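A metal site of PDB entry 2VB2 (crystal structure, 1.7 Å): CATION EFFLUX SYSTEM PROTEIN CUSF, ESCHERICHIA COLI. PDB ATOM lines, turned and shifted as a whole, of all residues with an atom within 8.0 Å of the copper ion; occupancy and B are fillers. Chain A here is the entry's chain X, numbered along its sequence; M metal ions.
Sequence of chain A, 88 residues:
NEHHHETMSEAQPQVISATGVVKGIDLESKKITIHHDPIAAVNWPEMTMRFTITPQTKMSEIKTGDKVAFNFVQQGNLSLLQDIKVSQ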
ATOM      1  N   ALA A  18      13.471  18.066 -17.335  1.00  0.00           N
ATOM      2  CA  ALA A  18      12.387  19.005 -17.165  1.00  0.00           C
ATOM      3  C   ALA A  18      11.140  18.538 -17.914  1.00  0.00           C
ATOM      4  O   ALA A  18      11.173  17.564 -18.665  1.00  0.00           O
ATOM      5  CB  ALA A  18      12.823  20.366 -17.653  1.00  0.00           C
ATOM      6  N   ILE A  34       9.986  26.469 -24.993  1.00  0.00           N
ATOM      7  CA  ILE A  34       9.233  25.647 -24.051  1.00  0.00           C
ATOM      8  C   ILE A  34       8.867  26.442 -22.810  1.00  0.00           C
ATOM      9  O   ILE A  34       9.723  27.064 -22.176  1.00  0.00           O
ATOM     10  CB  ILE A  34      10.037  24.395 -23.623  1.00  0.00           C
ATOM     11  CG1 ILE A  34      10.547  23.628 -24.856  1.00  0.00           C
ATOM     12  CG2 ILE A  34       9.201  23.466 -22.694  1.00  0.00           C
ATOM     13  CD1 ILE A  34      11.440  22.398 -24.487  1.00  0.00           C
ATOM     14  N   HIS A  35       7.578  26.385 -22.443  1.00  0.00           N
ATOM     15  CA  HIS A  35       7.149  26.879 -21.144  1.00  0.00           C
ATOM     16  C   HIS A  35       7.303  25.728 -20.161  1.00  0.00           C
ATOM     17  O   HIS A  35       6.484  24.794 -20.149  1.00  0.00           O
ATOM     18  CB  HIS A  35       5.702  27.376 -21.199  1.00  0.00           C
ATOM     19  CG  HIS A  35       5.219  27.988 -19.920  1.00  0.00           C
ATOM     20  ND1 HIS A  35       4.223  28.932 -19.880  1.00  0.00           N
ATOM     21  CD2 HIS A  35       5.601  27.770 -18.636  1.00  0.00           C
ATOM     22  CE1 HIS A  35       4.002  29.274 -18.624  1.00  0.00           C
ATOM     23  NE2 HIS A  35       4.821  28.584 -17.850  1.00  0.00           N
ATOM     24  N   HIS A  36       8.369  25.768 -19.370  1.00  0.00           N
ATOM     25  CA  HIS A  36       8.752  24.636 -18.544  1.00  0.00           C
ATOM     26  C   HIS A  36       8.214  24.751 -17.130  1.00  0.00           C
ATOM     27  O   HIS A  36       7.972  25.857 -16.636  1.00  0.00           O
ATOM     28  CB  HIS A  36      10.282  24.354 -18.599  1.00  0.00           C
ATOM     29  CG  HIS A  36      11.157  25.407 -17.967  1.00  0.00           C
ATOM     30  ND1 HIS A  36      11.251  25.577 -16.604  1.00  0.00           N
ATOM     31  CD2 HIS A  36      12.043  26.272 -18.512  1.00  0.00           C
ATOM     32  CE1 HIS A  36      12.122  26.543 -16.336  1.00  0.00           C
ATOM     33  NE2 HIS A  36      12.633  26.977 -17.480  1.00  0.00           N
ATOM     34  N   ASP A  37       7.971  23.598 -16.507  1.00  0.00           N
ATOM     35  CA  ASP A  37       7.531  23.503 -15.133  1.00  0.00           C
ATOM     36  C   ASP A  37       8.740  23.800 -14.251  1.00  0.00           C
ATOM     37  O   ASP A  37       9.869  23.787 -14.733  1.00  0.00           O
ATOM     38  CB  ASP A  37       6.995  22.102 -14.851  1.00  0.00           C
ATOM     39  CG  ASP A  37       5.714  21.807 -15.615  1.00  0.00           C
ATOM     40  OD1 ASP A  37       4.741  22.581 -15.464  1.00  0.00           O
ATOM     41  OD2 ASP A  37       5.680  20.814 -16.371  1.00  0.00           O
ATOM     42  N   PRO A  38       8.515  24.093 -12.951  1.00  0.00           N
ATOM     43  CA  PRO A  38       9.690  24.359 -12.115  1.00  0.00           C
ATOM     44  C   PRO A  38      10.727  23.244 -12.161  1.00  0.00           C
ATOM     45  O   PRO A  38      10.374  22.061 -12.253  1.00  0.00           O
ATOM     46  CB  PRO A  38       9.087  24.506 -10.713  1.00  0.00           C
ATOM     47  CG  PRO A  38       7.706  25.045 -11.000  1.00  0.00           C
ATOM     48  CD  PRO A  38       7.267  24.221 -12.170  1.00  0.00           C
ATOM     49  N   ILE A  39      11.989  23.644 -12.105  1.00  0.00           N
ATOM     50  CA  ILE A  39      13.094  22.704 -12.116  1.00  0.00           C
ATOM     51  C   ILE A  39      13.882  22.775 -10.800  1.00  0.00           C
ATOM     52  O   ILE A  39      14.715  23.663 -10.596  1.00  0.00           O
ATOM     53  CB  ILE A  39      14.048  22.933 -13.298  1.00  0.00           C
ATOM     54  CG1 ILE A  39      13.260  23.005 -14.619  1.00  0.00           C
ATOM     55  CG2 ILE A  39      15.062  21.809 -13.348  1.00  0.00           C
ATOM     56  CD1 ILE A  39      14.118  23.302 -15.855  1.00  0.00           C
ATOM     57  N   VAL A  42      18.029  23.046 -10.308  1.00  0.00           N
ATOM     58  CA  VAL A  42      18.677  24.332 -10.518  1.00  0.00           C
ATOM     59  C   VAL A  42      17.910  25.515  -9.885  1.00  0.00           C
ATOM     60  O   VAL A  42      18.280  26.682 -10.081  1.00  0.00           O
ATOM     61  CB  VAL A  42      18.953  24.594 -12.032  1.00  0.00           C
ATOM     62  CG1 VAL A  42      20.051  23.645 -12.539  1.00  0.00           C
ATOM     63  CG2 VAL A  42      17.684  24.428 -12.878  1.00  0.00           C
ATOM     64  N   TRP A  44      14.870  26.677 -10.414  1.00  0.00           N
ATOM     65  CA  TRP A  44      14.135  27.477 -11.397  1.00  0.00           C
ATOM     66  C   TRP A  44      12.638  27.363 -11.184  1.00  0.00           C
ATOM     67  O   TRP A  44      12.119  26.254 -11.022  1.00  0.00           O
ATOM     68  CB  TRP A  44      14.448  27.039 -12.828  1.00  0.00           C
ATOM     69  CG  TRP A  44      15.783  27.480 -13.375  1.00  0.00           C
ATOM     70  CD1 TRP A  44      16.768  28.173 -12.727  1.00  0.00           C
ATOM     71  CD2 TRP A  44      16.264  27.242 -14.699  1.00  0.00           C
ATOM     72  NE1 TRP A  44      17.845  28.369 -13.561  1.00  0.00           N
ATOM     73  CE2 TRP A  44      17.565  27.804 -14.780  1.00  0.00           C
ATOM     74  CE3 TRP A  44      15.738  26.598 -15.816  1.00  0.00           C
ATOM     75  CZ2 TRP A  44      18.341  27.744 -15.939  1.00  0.00           C
ATOM     76  CZ3 TRP A  44      16.522  26.538 -16.996  1.00  0.00           C
ATOM     77  CH2 TRP A  44      17.812  27.120 -17.033  1.00  0.00           C
ATOM     78  N   PRO A  45      11.927  28.501 -11.224  1.00  0.00           N
ATOM     79  CA  PRO A  45      10.474  28.471 -11.214  1.00  0.00           C
ATOM     80  C   PRO A  45      10.023  28.124 -12.622  1.00  0.00           C
ATOM     81  O   PRO A  45      10.856  27.871 -13.494  1.00  0.00           O
ATOM     82  CB  PRO A  45      10.098  29.922 -10.868  1.00  0.00           C
ATOM     83  CG  PRO A  45      11.211  30.726 -11.454  1.00  0.00           C
ATOM     84  CD  PRO A  45      12.460  29.875 -11.323  1.00  0.00           C
ATOM     85  N   GLU A  46       8.721  28.102 -12.863  1.00  0.00           N
ATOM     86  CA  GLU A  46       8.248  27.993 -14.242  1.00  0.00           C
ATOM     87  C   GLU A  46       8.789  29.176 -15.060  1.00  0.00           C
ATOM     88  O   GLU A  46       8.748  30.332 -14.618  1.00  0.00           O
ATOM     89  CB  GLU A  46       6.720  27.903 -14.303  1.00  0.00           C
ATOM     90  CG  GLU A  46       5.974  29.144 -13.888  1.00  0.00           C
ATOM     91  CD  GLU A  46       4.480  28.989 -14.058  1.00  0.00           C
ATOM     92  OE1 GLU A  46       3.779  28.989 -13.036  1.00  0.00           O
ATOM     93  OE2 GLU A  46       4.007  28.849 -15.206  1.00  0.00           O
ATOM     94  N   MET A  47       9.338  28.884 -16.235  1.00  0.00           N
ATOM     95  CA  MET A  47       9.773  29.908 -17.194  1.00  0.00           C
ATOM     96  C   MET A  47       9.398  29.473 -18.593  1.00  0.00           C
ATOM     97  O   MET A  47       9.164  28.298 -18.838  1.00  0.00           O
ATOM     98  CB  MET A  47      11.300  30.073 -17.240  1.00  0.00           C
ATOM     99  CG  MET A  47      12.054  30.299 -15.949  1.00  0.00           C
ATOM    100  SD  MET A  47      13.846  30.107 -16.242  1.00  0.00           S
ATOM    101  CE  MET A  47      14.410  30.335 -14.577  1.00  0.00           C
ATOM    102  N   THR A  48       9.430  30.434 -19.514  1.00  0.00           N
ATOM    103  CA  THR A  48       9.506  30.174 -20.926  1.00  0.00           C
ATOM    104  C   THR A  48      10.956  30.426 -21.393  1.00  0.00           C
ATOM    105  O   THR A  48      11.529  31.473 -21.116  1.00  0.00           O
ATOM    106  CB  THR A  48       8.513  31.067 -21.725  1.00  0.00           C
ATOM    107  OG1 THR A  48       7.190  30.827 -21.243  1.00  0.00           O
ATOM    108  CG2 THR A  48       8.573  30.747 -23.192  1.00  0.00           C
ATOM    109  N   MET A  49      11.538  29.442 -22.083  1.00  0.00           N
ATOM    110  CA  MET A  49      12.921  29.516 -22.560  1.00  0.00           C
ATOM    111  C   MET A  49      13.030  28.881 -23.926  1.00  0.00           C
ATOM    112  O   MET A  49      12.241  28.005 -24.252  1.00  0.00           O
ATOM    113  CB  MET A  49      13.839  28.716 -21.641  1.00  0.00           C
ATOM    114  CG  MET A  49      13.733  29.038 -20.195  1.00  0.00           C
ATOM    115  SD  MET A  49      15.132  28.256 -19.380  1.00  0.00           S
ATOM    116  CE  MET A  49      16.320  29.578 -19.507  1.00  0.00           C
ATOM    117  N   ARG A  50      14.022  29.289 -24.725  1.00  0.00           N
ATOM    118  CA  ARG A  50      14.324  28.560 -25.957  1.00  0.00           C
ATOM    119  C   ARG A  50      15.414  27.537 -25.688  1.00  0.00           C
ATOM    120  O   ARG A  50      16.449  27.846 -25.079  1.00  0.00           O
ATOM    121  CB  ARG A  50      14.758  29.475 -27.106  1.00  0.00           C
ATOM    122  CG  ARG A  50      13.697  30.511 -27.516  1.00  0.00           C
ATOM    123  CD  ARG A  50      13.877  30.963 -28.976  1.00  0.00           C
ATOM    124  NE  ARG A  50      15.181  31.585 -29.220  1.00  0.00           N
ATOM    125  CZ  ARG A  50      15.443  32.422 -30.232  1.00  0.00           C
ATOM    126  NH1 ARG A  50      14.497  32.757 -31.109  1.00  0.00           N
ATOM    127  NH2 ARG A  50      16.664  32.934 -30.365  1.00  0.00           N
ATOM    128  N   PHE A  51      15.176  26.325 -26.167  1.00  0.00           N
ATOM    129  CA  PHE A  51      16.145  25.240 -26.027  1.00  0.00           C
ATOM    130  C   PHE A  51      16.699  24.875 -27.392  1.00  0.00           C
ATOM    131  O   PHE A  51      15.966  24.717 -28.384  1.00  0.00           O
ATOM    132  CB  PHE A  51      15.483  24.068 -25.321  1.00  0.00           C
ATOM    133  CG  PHE A  51      15.116  24.356 -23.890  1.00  0.00           C
ATOM    134  CD1 PHE A  51      13.888  24.955 -23.573  1.00  0.00           C
ATOM    135  CD2 PHE A  51      16.004  24.086 -22.864  1.00  0.00           C
ATOM    136  CE1 PHE A  51      13.548  25.231 -22.261  1.00  0.00           C
ATOM    137  CE2 PHE A  51      15.679  24.362 -21.533  1.00  0.00           C
ATOM    138  CZ  PHE A  51      14.454  24.948 -21.234  1.00  0.00           C
ATOM    139  N   PHE A  70      11.878  16.488 -21.408  1.00  0.00           N
ATOM    140  CA  PHE A  70      13.136  16.764 -22.087  1.00  0.00           C
ATOM    141  C   PHE A  70      14.319  16.816 -21.123  1.00  0.00           C
ATOM    142  O   PHE A  70      14.140  16.994 -19.905  1.00  0.00           O
ATOM    143  CB  PHE A  70      13.055  18.049 -22.945  1.00  0.00           C
ATOM    144  CG  PHE A  70      12.763  19.306 -22.174  1.00  0.00           C
ATOM    145  CD1 PHE A  70      13.766  20.217 -21.915  1.00  0.00           C
ATOM    146  CD2 PHE A  70      11.466  19.576 -21.732  1.00  0.00           C
ATOM    147  CE1 PHE A  70      13.511  21.387 -21.214  1.00  0.00           C
ATOM    148  CE2 PHE A  70      11.186  20.749 -21.016  1.00  0.00           C
ATOM    149  CZ  PHE A  70      12.223  21.655 -20.769  1.00  0.00           C
ATOM    150  N   PHE A  72      18.292  18.575 -20.767  1.00  0.00           N
ATOM    151  CA  PHE A  72      19.218  19.552 -21.327  1.00  0.00           C
ATOM    152  C   PHE A  72      20.462  19.792 -20.487  1.00  0.00           C
ATOM    153  O   PHE A  72      20.513  19.404 -19.319  1.00  0.00           O
ATOM    154  CB  PHE A  72      18.519  20.911 -21.644  1.00  0.00           C
ATOM    155  CG  PHE A  72      18.083  21.690 -20.432  1.00  0.00           C
ATOM    156  CD1 PHE A  72      18.864  22.749 -19.965  1.00  0.00           C
ATOM    157  CD2 PHE A  72      16.896  21.403 -19.777  1.00  0.00           C
ATOM    158  CE1 PHE A  72      18.494  23.505 -18.836  1.00  0.00           C
ATOM    159  CE2 PHE A  72      16.504  22.159 -18.646  1.00  0.00           C
ATOM    160  CZ  PHE A  72      17.300  23.201 -18.170  1.00  0.00           C
ATOM    161  N   GLN A  74      23.361  23.075 -19.615  1.00  0.00           N
ATOM    162  CA  GLN A  74      23.683  24.482 -19.706  1.00  0.00           C
ATOM    163  C   GLN A  74      25.089  24.565 -20.278  1.00  0.00           C
ATOM    164  O   GLN A  74      26.029  24.038 -19.665  1.00  0.00           O
ATOM    165  CB  GLN A  74      23.633  25.128 -18.318  1.00  0.00           C
ATOM    166  CG  GLN A  74      22.414  24.716 -17.489  1.00  0.00           C
ATOM    167  CD  GLN A  74      22.282  25.494 -16.187  1.00  0.00           C
ATOM    168  OE1 GLN A  74      22.594  24.981 -15.108  1.00  0.00           O
ATOM    169  NE2 GLN A  74      21.828  26.733 -16.287  1.00  0.00           N
ATOM    170  N   SER A  79      20.919  26.674 -23.782  1.00  0.00           N
ATOM    171  CA  SER A  79      20.414  25.471 -23.146  1.00  0.00           C
ATOM    172  C   SER A  79      20.353  24.408 -24.217  1.00  0.00           C
ATOM    173  O   SER A  79      19.472  24.428 -25.074  1.00  0.00           O
ATOM    174  CB  SER A  79      19.009  25.723 -22.590  1.00  0.00           C
ATOM    175  OG  SER A  79      19.012  26.966 -21.902  1.00  0.00           O
HETATM  176 CU    CU M   1      14.197  28.176 -17.329  1.00  0.00          CU
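CE3 of Trp 44 touches the copper ion, at 2.7 Å. Within 4 Å of the copper ion: His 36, Trp 44, Met 47 and Met 49. Along chain A the residues within 4 Å of the copper ion span positions 36 to 49. The nearest printed residue that does not touch the copper ion is Phe 51 (5.1 Å).
NE2 of His 36 binds the copper ion. The copper ion is bound by SD of Met 47 (2.2 Å). The side-chain sulfur (SD) of Met 49 binds the copper ion, 2.3 Å away. The copper ion has three donor atoms within binding distance.
The backbone NH (N) of Ile 34 is in hydrogen-bond range of the backbone carbonyl oxygen (O) of Met 49. The backbone carbonyl oxygen (O) of Trp 44 sits at hydrogen-bond distance from the backbone NH (N) of Ile 39 (2.8 Å).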
